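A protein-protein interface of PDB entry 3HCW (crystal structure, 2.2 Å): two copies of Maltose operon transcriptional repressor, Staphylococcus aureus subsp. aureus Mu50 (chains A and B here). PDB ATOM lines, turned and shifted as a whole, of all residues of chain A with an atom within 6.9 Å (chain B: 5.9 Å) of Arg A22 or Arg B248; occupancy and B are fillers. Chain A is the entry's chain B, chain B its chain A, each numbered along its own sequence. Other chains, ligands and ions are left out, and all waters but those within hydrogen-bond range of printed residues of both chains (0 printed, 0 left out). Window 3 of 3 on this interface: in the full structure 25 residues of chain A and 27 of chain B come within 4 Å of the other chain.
Ile B28 touches its own counterpart, Ile A28.
Position printed for both chains: 28.
Among the printed residues, pairs that only touch across the chains: Arg A22 with Ile B28 (3.8 Å), Arg A22 with Leu B32 (3.6 Å), Arg A22 with Arg B248 (3.7 Å), Leu A23 with Ile B28 (3.7 Å) and Ile A28 with Ile B28 (3.6 Å).
Hydrophobic or aromatic side chains of chain A within 4 Å of the printed part of chain B: Leu A23 and Ile A28.
Of the 15 printed residues of chain B, 4 touch a printed residue of chain A.
Hydrophobic or aromatic side chains of chain B that line the printed part of chain A: Ile B28 and Leu B32.
Among the printed residues, 7 pairs touch across the chains.
Among the printed residues, no Asp or Glu carboxylate lies within 4 Å of a Lys or Arg side-chain nitrogen of the other chain.
The side-chain carboxylate (OE1) of Glu A19 lies within salt-bridge range of the guanidinium group (NH2) of Arg A22, 3.8 Å away.
The backbone carbonyl oxygen (O) of Ser A17 lies within hydrogen-bond range of the guanidinium group (NH1) of Arg A22 (2.7 Å).
The side-chain carboxylate (OE2) of Glu B36 is in salt-bridge range of the guanidinium group (NH1) of Arg B248 (2.7 Å).
NH2 of Arg A22 lies within hydrogen-bond range of OD1 of Asn B29, at 2.7 Å.
The side-chain amide nitrogen (ND2) of Asn B29 sits at hydrogen-bond distance from the side-chain carboxylate (OE1) of Glu A19.
Of the printed residues of chain B, Glu A19 touches Asn B29.
Of chain B, only Ile B28, Asn B29, Leu B32 and Arg B248 come within 4 Å of Arg A22.
Of the printed residues of chain B, Leu A23 touches Ile B28 (3.7 Å).
Printed residues of chain B within 4 Å of Ile A28: Ile B28 (3.6 Å).
Leu A31 touches none of the printed residues of chain B.
Printed residues of chain A within 4 Å of Ile B28: Arg A22 (3.8 Å), Leu A23 (3.7 Å) and Ile A28 (3.6 Å).
Printed residues of chain A within 4 Å of Leu B32: Arg A22 (3.6 Å).
Ile B34 touches none of the printed residues of chain A.
Arg B248 touches just one residue of chain A: Arg A22 (3.7 Å).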
ATOM      1  N   LEU A  14     -30.737  33.401  23.426  1.00  0.00           N
ATOM      2  CA  LEU A  14     -29.476  33.998  23.900  1.00  0.00           C
ATOM      3  C   LEU A  14     -29.145  35.282  23.123  1.00  0.00           C
ATOM      4  O   LEU A  14     -29.702  35.530  22.057  1.00  0.00           O
ATOM      5  CB  LEU A  14     -28.318  32.997  23.784  1.00  0.00           C
ATOM      6  CG  LEU A  14     -28.261  31.807  24.756  1.00  0.00           C
ATOM      7  CD1 LEU A  14     -29.097  30.639  24.274  1.00  0.00           C
ATOM      8  CD2 LEU A  14     -26.838  31.335  24.965  1.00  0.00           C
ATOM      9  N   GLY A  16     -26.222  36.078  21.811  1.00  0.00           N
ATOM     10  CA  GLY A  16     -25.355  35.706  20.697  1.00  0.00           C
ATOM     11  C   GLY A  16     -24.932  34.257  20.840  1.00  0.00           C
ATOM     12  O   GLY A  16     -25.286  33.591  21.810  1.00  0.00           O
ATOM     13  N   SER A  17     -24.173  33.761  19.872  1.00  0.00           N
ATOM     14  CA  SER A  17     -23.789  32.359  19.876  1.00  0.00           C
ATOM     15  C   SER A  17     -22.307  32.180  19.604  1.00  0.00           C
ATOM     16  O   SER A  17     -21.832  31.054  19.471  1.00  0.00           O
ATOM     17  CB  SER A  17     -24.601  31.583  18.841  1.00  0.00           C
ATOM     18  OG  SER A  17     -24.181  31.923  17.534  1.00  0.00           O
ATOM     19  N   GLU A  18     -21.575  33.288  19.522  1.00  0.00           N
ATOM     20  CA  GLU A  18     -20.133  33.238  19.332  1.00  0.00           C
ATOM     21  C   GLU A  18     -19.462  32.541  20.521  1.00  0.00           C
ATOM     22  O   GLU A  18     -20.091  32.319  21.558  1.00  0.00           O
ATOM     23  CB  GLU A  18     -19.578  34.643  19.140  1.00  0.00           C
ATOM     24  CG  GLU A  18     -19.833  35.586  20.305  1.00  0.00           C
ATOM     25  CD  GLU A  18     -18.947  36.814  20.253  1.00  0.00           C
ATOM     26  OE1 GLU A  18     -18.597  37.250  19.133  1.00  0.00           O
ATOM     27  OE2 GLU A  18     -18.601  37.343  21.332  1.00  0.00           O
ATOM     28  N   GLU A  19     -18.195  32.180  20.390  1.00  0.00           N
ATOM     29  CA  GLU A  19     -17.602  31.415  21.484  1.00  0.00           C
ATOM     30  C   GLU A  19     -17.333  32.075  22.857  1.00  0.00           C
ATOM     31  O   GLU A  19     -17.389  31.373  23.863  1.00  0.00           O
ATOM     32  CB  GLU A  19     -16.525  30.410  21.046  1.00  0.00           C
ATOM     33  CG  GLU A  19     -15.570  30.742  19.944  1.00  0.00           C
ATOM     34  CD  GLU A  19     -14.524  29.632  19.793  1.00  0.00           C
ATOM     35  OE1 GLU A  19     -14.897  28.432  19.725  1.00  0.00           O
ATOM     36  OE2 GLU A  19     -13.324  29.957  19.761  1.00  0.00           O
ATOM     37  N   PRO A  20     -17.065  33.404  22.926  1.00  0.00           N
ATOM     38  CA  PRO A  20     -17.154  34.028  24.267  1.00  0.00           C
ATOM     39  C   PRO A  20     -18.486  33.784  25.005  1.00  0.00           C
ATOM     40  O   PRO A  20     -18.505  33.674  26.237  1.00  0.00           O
ATOM     41  CB  PRO A  20     -16.971  35.515  23.973  1.00  0.00           C
ATOM     42  CG  PRO A  20     -16.122  35.535  22.749  1.00  0.00           C
ATOM     43  CD  PRO A  20     -16.606  34.377  21.915  1.00  0.00           C
ATOM     44  N   ILE A  21     -19.577  33.680  24.253  1.00  0.00           N
ATOM     45  CA  ILE A  21     -20.875  33.322  24.824  1.00  0.00           C
ATOM     46  C   ILE A  21     -21.058  31.796  24.947  1.00  0.00           C
ATOM     47  O   ILE A  21     -21.232  31.281  26.043  1.00  0.00           O
ATOM     48  CB  ILE A  21     -22.021  33.991  24.045  1.00  0.00           C
ATOM     49  CG1 ILE A  21     -21.994  35.503  24.319  1.00  0.00           C
ATOM     50  CG2 ILE A  21     -23.360  33.397  24.437  1.00  0.00           C
ATOM     51  CD1 ILE A  21     -22.604  36.372  23.229  1.00  0.00           C
ATOM     52  N   ARG A  22     -20.967  31.068  23.837  1.00  0.00           N
ATOM     53  CA  ARG A  22     -21.337  29.650  23.852  1.00  0.00           C
ATOM     54  C   ARG A  22     -20.364  28.730  24.605  1.00  0.00           C
ATOM     55  O   ARG A  22     -20.739  27.615  24.953  1.00  0.00           O
ATOM     56  CB  ARG A  22     -21.605  29.132  22.436  1.00  0.00           C
ATOM     57  CG  ARG A  22     -20.356  28.895  21.611  1.00  0.00           C
ATOM     58  CD  ARG A  22     -20.695  28.082  20.396  1.00  0.00           C
ATOM     59  NE  ARG A  22     -19.535  27.881  19.537  1.00  0.00           N
ATOM     60  CZ  ARG A  22     -19.251  28.599  18.455  1.00  0.00           C
ATOM     61  NH1 ARG A  22     -20.043  29.590  18.068  1.00  0.00           N
ATOM     62  NH2 ARG A  22     -18.170  28.298  17.742  1.00  0.00           N
ATOM     63  N   LEU A  23     -19.131  29.196  24.844  1.00  0.00           N
ATOM     64  CA  LEU A  23     -18.148  28.442  25.650  1.00  0.00           C
ATOM     65  C   LEU A  23     -18.179  28.809  27.131  1.00  0.00           C
ATOM     66  O   LEU A  23     -17.481  28.177  27.940  1.00  0.00           O
ATOM     67  CB  LEU A  23     -16.721  28.607  25.121  1.00  0.00           C
ATOM     68  CG  LEU A  23     -16.405  28.199  23.678  1.00  0.00           C
ATOM     69  CD1 LEU A  23     -14.910  28.300  23.405  1.00  0.00           C
ATOM     70  CD2 LEU A  23     -16.933  26.823  23.329  1.00  0.00           C
ATOM     71  N   ASN A  24     -18.982  29.826  27.464  1.00  0.00           N
ATOM     72  CA  ASN A  24     -19.203  30.267  28.846  1.00  0.00           C
ATOM     73  C   ASN A  24     -20.035  29.229  29.566  1.00  0.00           C
ATOM     74  O   ASN A  24     -21.189  28.994  29.193  1.00  0.00           O
ATOM     75  CB  ASN A  24     -19.927  31.617  28.856  1.00  0.00           C
ATOM     76  CG  ASN A  24     -19.750  32.386  30.157  1.00  0.00           C
ATOM     77  OD1 ASN A  24     -19.421  31.824  31.197  1.00  0.00           O
ATOM     78  ND2 ASN A  24     -19.971  33.695  30.093  1.00  0.00           N
ATOM     79  N   PRO A  25     -19.456  28.601  30.600  1.00  0.00           N
ATOM     80  CA  PRO A  25     -20.153  27.575  31.384  1.00  0.00           C
ATOM     81  C   PRO A  25     -21.423  28.062  32.088  1.00  0.00           C
ATOM     82  O   PRO A  25     -22.198  27.228  32.573  1.00  0.00           O
ATOM     83  CB  PRO A  25     -19.109  27.157  32.422  1.00  0.00           C
ATOM     84  CG  PRO A  25     -17.789  27.540  31.810  1.00  0.00           C
ATOM     85  CD  PRO A  25     -18.080  28.814  31.089  1.00  0.00           C
ATOM     86  N   TYR A  27     -23.856  29.936  30.419  1.00  0.00           N
ATOM     87  CA  TYR A  27     -24.850  29.620  29.414  1.00  0.00           C
ATOM     88  C   TYR A  27     -24.954  28.128  29.154  1.00  0.00           C
ATOM     89  O   TYR A  27     -26.056  27.617  29.000  1.00  0.00           O
ATOM     90  CB  TYR A  27     -24.631  30.398  28.126  1.00  0.00           C
ATOM     91  CG  TYR A  27     -24.745  31.882  28.335  1.00  0.00           C
ATOM     92  CD1 TYR A  27     -25.968  32.469  28.640  1.00  0.00           C
ATOM     93  CD2 TYR A  27     -23.628  32.704  28.231  1.00  0.00           C
ATOM     94  CE1 TYR A  27     -26.073  33.838  28.843  1.00  0.00           C
ATOM     95  CE2 TYR A  27     -23.725  34.076  28.425  1.00  0.00           C
ATOM     96  CZ  TYR A  27     -24.948  34.633  28.730  1.00  0.00           C
ATOM     97  OH  TYR A  27     -25.039  35.985  28.933  1.00  0.00           O
ATOM     98  N   ILE A  28     -23.820  27.434  29.144  1.00  0.00           N
ATOM     99  CA  ILE A  28     -23.812  25.979  28.968  1.00  0.00           C
ATOM    100  C   ILE A  28     -24.589  25.319  30.095  1.00  0.00           C
ATOM    101  O   ILE A  28     -25.436  24.472  29.839  1.00  0.00           O
ATOM    102  CB  ILE A  28     -22.386  25.395  28.905  1.00  0.00           C
ATOM    103  CG1 ILE A  28     -21.629  25.965  27.709  1.00  0.00           C
ATOM    104  CG2 ILE A  28     -22.427  23.866  28.796  1.00  0.00           C
ATOM    105  CD1 ILE A  28     -20.143  25.945  27.893  1.00  0.00           C
ATOM    106  N   LEU A  31     -28.491  26.251  30.056  1.00  0.00           N
ATOM    107  CA  LEU A  31     -29.104  25.517  28.945  1.00  0.00           C
ATOM    108  C   LEU A  31     -29.262  24.028  29.258  1.00  0.00           C
ATOM    109  O   LEU A  31     -30.286  23.442  28.923  1.00  0.00           O
ATOM    110  CB  LEU A  31     -28.331  25.715  27.625  1.00  0.00           C
ATOM    111  CG  LEU A  31     -28.401  27.069  26.883  1.00  0.00           C
ATOM    112  CD1 LEU A  31     -27.339  27.190  25.765  1.00  0.00           C
ATOM    113  CD2 LEU A  31     -29.773  27.350  26.313  1.00  0.00           C
ATOM    114  N   VAL A  49     -29.517  30.647  17.246  1.00  0.00           N
ATOM    115  CA  VAL A  49     -28.143  30.549  16.732  1.00  0.00           C
ATOM    116  C   VAL A  49     -27.560  31.886  16.255  1.00  0.00           C
ATOM    117  O   VAL A  49     -26.382  31.957  15.922  1.00  0.00           O
ATOM    118  CB  VAL A  49     -27.981  29.486  15.596  1.00  0.00           C
ATOM    119  CG1 VAL A  49     -26.763  28.611  15.873  1.00  0.00           C
ATOM    120  CG2 VAL A  49     -29.216  28.609  15.447  1.00  0.00           C
ATOM    121  N   MET A 202     -15.544  35.167  32.224  1.00  0.00           N
ATOM    122  CA  MET A 202     -14.992  35.176  30.871  1.00  0.00           C
ATOM    123  C   MET A 202     -14.220  36.465  30.567  1.00  0.00           C
ATOM    124  O   MET A 202     -13.119  36.394  30.027  1.00  0.00           O
ATOM    125  CB  MET A 202     -16.079  34.897  29.821  1.00  0.00           C
ATOM    126  CG  MET A 202     -15.532  34.461  28.454  1.00  0.00           C
ATOM    127  SD  MET A 202     -14.647  32.876  28.472  1.00  0.00           S
ATOM    128  CE  MET A 202     -16.012  31.742  28.507  1.00  0.00           C
ATOM    129  N   ILE B  28     -18.394  21.225  22.452  1.00  0.00           N
ATOM    130  CA  ILE B  28     -19.347  22.319  22.171  1.00  0.00           C
ATOM    131  C   ILE B  28     -19.389  22.667  20.678  1.00  0.00           C
ATOM    132  O   ILE B  28     -20.461  22.733  20.082  1.00  0.00           O
ATOM    133  CB  ILE B  28     -19.075  23.569  23.034  1.00  0.00           C
ATOM    134  CG1 ILE B  28     -19.333  23.236  24.506  1.00  0.00           C
ATOM    135  CG2 ILE B  28     -19.959  24.757  22.589  1.00  0.00           C
ATOM    136  CD1 ILE B  28     -18.472  23.991  25.429  1.00  0.00           C
ATOM    137  N   ASN B  29     -18.221  22.821  20.064  1.00  0.00           N
ATOM    138  CA  ASN B  29     -18.176  23.114  18.640  1.00  0.00           C
ATOM    139  C   ASN B  29     -18.513  21.937  17.723  1.00  0.00           C
ATOM    140  O   ASN B  29     -19.153  22.131  16.691  1.00  0.00           O
ATOM    141  CB  ASN B  29     -16.850  23.769  18.278  1.00  0.00           C
ATOM    142  CG  ASN B  29     -16.703  25.142  18.905  1.00  0.00           C
ATOM    143  OD1 ASN B  29     -17.634  25.935  18.883  1.00  0.00           O
ATOM    144  ND2 ASN B  29     -15.537  25.423  19.475  1.00  0.00           N
ATOM    145  N   VAL B  30     -18.113  20.723  18.100  1.00  0.00           N
ATOM    146  CA  VAL B  30     -18.444  19.539  17.288  1.00  0.00           C
ATOM    147  C   VAL B  30     -19.959  19.323  17.268  1.00  0.00           C
ATOM    148  O   VAL B  30     -20.555  19.212  16.186  1.00  0.00           O
ATOM    149  CB  VAL B  30     -17.671  18.260  17.727  1.00  0.00           C
ATOM    150  CG1 VAL B  30     -18.191  17.058  17.013  1.00  0.00           C
ATOM    151  CG2 VAL B  30     -16.196  18.389  17.400  1.00  0.00           C
ATOM    152  N   LEU B  32     -22.330  21.590  17.991  1.00  0.00           N
ATOM    153  CA  LEU B  32     -22.897  22.701  17.198  1.00  0.00           C
ATOM    154  C   LEU B  32     -22.796  22.455  15.683  1.00  0.00           C
ATOM    155  O   LEU B  32     -23.762  22.670  14.936  1.00  0.00           O
ATOM    156  CB  LEU B  32     -22.224  24.035  17.560  1.00  0.00           C
ATOM    157  CG  LEU B  32     -22.724  25.314  16.876  1.00  0.00           C
ATOM    158  CD1 LEU B  32     -24.116  25.698  17.356  1.00  0.00           C
ATOM    159  CD2 LEU B  32     -21.767  26.457  17.112  1.00  0.00           C
ATOM    160  N   GLY B  33     -21.627  22.000  15.239  1.00  0.00           N
ATOM    161  CA  GLY B  33     -21.422  21.620  13.852  1.00  0.00           C
ATOM    162  C   GLY B  33     -22.397  20.543  13.405  1.00  0.00           C
ATOM    163  O   GLY B  33     -23.044  20.689  12.362  1.00  0.00           O
ATOM    164  N   ILE B  34     -22.522  19.470  14.195  1.00  0.00           N
ATOM    165  CA  ILE B  34     -23.469  18.403  13.865  1.00  0.00           C
ATOM    166  C   ILE B  34     -24.920  18.897  13.836  1.00  0.00           C
ATOM    167  O   ILE B  34     -25.631  18.674  12.859  1.00  0.00           O
ATOM    168  CB  ILE B  34     -23.383  17.217  14.848  1.00  0.00           C
ATOM    169  CG1 ILE B  34     -22.042  16.506  14.716  1.00  0.00           C
ATOM    170  CG2 ILE B  34     -24.550  16.220  14.593  1.00  0.00           C
ATOM    171  CD1 ILE B  34     -21.564  15.881  15.973  1.00  0.00           C
ATOM    172  N   GLU B  36     -26.514  21.975  13.763  1.00  0.00           N
ATOM    173  CA  GLU B  36     -26.973  22.965  12.789  1.00  0.00           C
ATOM    174  C   GLU B  36     -27.138  22.361  11.388  1.00  0.00           C
ATOM    175  O   GLU B  36     -28.085  22.695  10.689  1.00  0.00           O
ATOM    176  CB  GLU B  36     -26.094  24.226  12.788  1.00  0.00           C
ATOM    177  CG  GLU B  36     -24.764  24.128  12.049  1.00  0.00           C
ATOM    178  CD  GLU B  36     -23.733  25.131  12.552  1.00  0.00           C
ATOM    179  OE1 GLU B  36     -22.532  24.781  12.600  1.00  0.00           O
ATOM    180  OE2 GLU B  36     -24.125  26.262  12.909  1.00  0.00           O
ATOM    181  N   LYS B 246     -10.341  22.651  13.880  1.00  0.00           N
ATOM    182  CA  LYS B 246     -11.618  22.932  13.218  1.00  0.00           C
ATOM    183  C   LYS B 246     -12.790  22.043  13.687  1.00  0.00           C
ATOM    184  O   LYS B 246     -13.361  21.291  12.882  1.00  0.00           O
ATOM    185  CB  LYS B 246     -11.450  22.833  11.695  1.00  0.00           C
ATOM    186  CG  LYS B 246     -10.134  23.379  11.142  1.00  0.00           C
ATOM    187  CD  LYS B 246     -10.138  24.901  11.047  1.00  0.00           C
ATOM    188  CE  LYS B 246      -8.749  25.412  10.688  1.00  0.00           C
ATOM    189  NZ  LYS B 246      -8.598  26.864  10.998  1.00  0.00           N
ATOM    190  N   PRO B 247     -13.138  22.106  14.987  1.00  0.00           N
ATOM    191  CA  PRO B 247     -14.183  21.201  15.510  1.00  0.00           C
ATOM    192  C   PRO B 247     -15.596  21.449  14.943  1.00  0.00           C
ATOM    193  O   PRO B 247     -16.389  20.501  14.801  1.00  0.00           O
ATOM    194  CB  PRO B 247     -14.115  21.416  17.031  1.00  0.00           C
ATOM    195  CG  PRO B 247     -13.485  22.783  17.209  1.00  0.00           C
ATOM    196  CD  PRO B 247     -12.570  22.982  16.035  1.00  0.00           C
ATOM    197  N   ARG B 248     -15.895  22.697  14.588  1.00  0.00           N
ATOM    198  CA  ARG B 248     -17.176  23.014  13.958  1.00  0.00           C
ATOM    199  C   ARG B 248     -17.258  22.413  12.555  1.00  0.00           C
ATOM    200  O   ARG B 248     -18.314  21.903  12.167  1.00  0.00           O
ATOM    201  CB  ARG B 248     -17.434  24.514  13.934  1.00  0.00           C
ATOM    202  CG  ARG B 248     -18.887  24.859  13.716  1.00  0.00           C
ATOM    203  CD  ARG B 248     -19.132  26.326  13.963  1.00  0.00           C
ATOM    204  NE  ARG B 248     -20.484  26.693  13.565  1.00  0.00           N
ATOM    205  CZ  ARG B 248     -21.041  27.873  13.798  1.00  0.00           C
ATOM    206  NH1 ARG B 248     -22.283  28.107  13.390  1.00  0.00           N
ATOM    207  NH2 ARG B 248     -20.359  28.815  14.430  1.00  0.00           N
ATOM    208  N   MET B 249     -16.137  22.447  11.825  1.00  0.00           N
ATOM    209  CA  MET B 249     -16.015  21.776  10.527  1.00  0.00           C
ATOM    210  C   MET B 249     -16.157  20.261  10.660  1.00  0.00           C
ATOM    211  O   MET B 249     -16.889  19.648   9.900  1.00  0.00           O
ATOM    212  CB  MET B 249     -14.677  22.093   9.855  1.00  0.00           C
ATOM    213  CG  MET B 249     -14.736  23.117   8.732  1.00  0.00           C
ATOM    214  SD  MET B 249     -13.225  23.122   7.730  1.00  0.00           S
ATOM    215  CE  MET B 249     -13.462  21.656   6.731  1.00  0.00           C
ATOM    216  N   LEU B 250     -15.440  19.663  11.617  1.00  0.00           N
ATOM    217  CA  LEU B 250     -15.561  18.218  11.876  1.00  0.00           C
ATOM    218  C   LEU B 250     -17.018  17.790  12.084  1.00  0.00           C
ATOM    219  O   LEU B 250     -17.464  16.793  11.521  1.00  0.00           O
ATOM    220  CB  LEU B 250     -14.742  17.815  13.114  1.00  0.00           C
ATOM    221  CG  LEU B 250     -13.219  17.762  13.031  1.00  0.00           C
ATOM    222  CD1 LEU B 250     -12.623  17.989  14.407  1.00  0.00           C
ATOM    223  CD2 LEU B 250     -12.733  16.436  12.446  1.00  0.00           C
ATOM    224  N   GLY B 251     -17.751  18.575  12.879  1.00  0.00           N
ATOM    225  CA  GLY B 251     -19.153  18.314  13.174  1.00  0.00           C
ATOM    226  C   GLY B 251     -20.060  18.444  11.959  1.00  0.00           C
ATOM    227  O   GLY B 251     -20.917  17.584  11.719  1.00  0.00           O
ATOM    228  N   GLN B 252     -19.869  19.515  11.192  1.00  0.00           N
ATOM    229  CA  GLN B 252     -20.641  19.732   9.968  1.00  0.00           C
ATOM    230  C   GLN B 252     -20.432  18.585   8.985  1.00  0.00           C
ATOM    231  O   GLN B 252     -21.392  18.104   8.398  1.00  0.00           O
ATOM    232  CB  GLN B 252     -20.289  21.071   9.312  1.00  0.00           C
ATOM    233  CG  GLN B 252     -20.823  22.279  10.064  1.00  0.00           C
ATOM    234  CD  GLN B 252     -20.295  23.603   9.518  1.00  0.00           C
ATOM    235  OE1 GLN B 252     -19.453  23.632   8.621  1.00  0.00           O
ATOM    236  NE2 GLN B 252     -20.798  24.706  10.063  1.00  0.00           N
ATOM    237  N   GLN B 253     -19.182  18.149   8.832  1.00  0.00           N
ATOM    238  CA  GLN B 253     -18.838  17.032   7.937  1.00  0.00           C
ATOM    239  C   GLN B 253     -19.443  15.695   8.398  1.00  0.00           C
ATOM    240  O   GLN B 253     -19.890  14.900   7.578  1.00  0.00           O
ATOM    241  CB  GLN B 253     -17.323  16.900   7.808  1.00  0.00           C
ATOM    242  CG  GLN B 253     -16.635  18.057   7.080  1.00  0.00           C
ATOM    243  CD  GLN B 253     -16.902  18.058   5.587  1.00  0.00           C
ATOM    244  OE1 GLN B 253     -16.749  17.035   4.913  1.00  0.00           O
ATOM    245  NE2 GLN B 253     -17.297  19.210   5.060  1.00  0.00           N
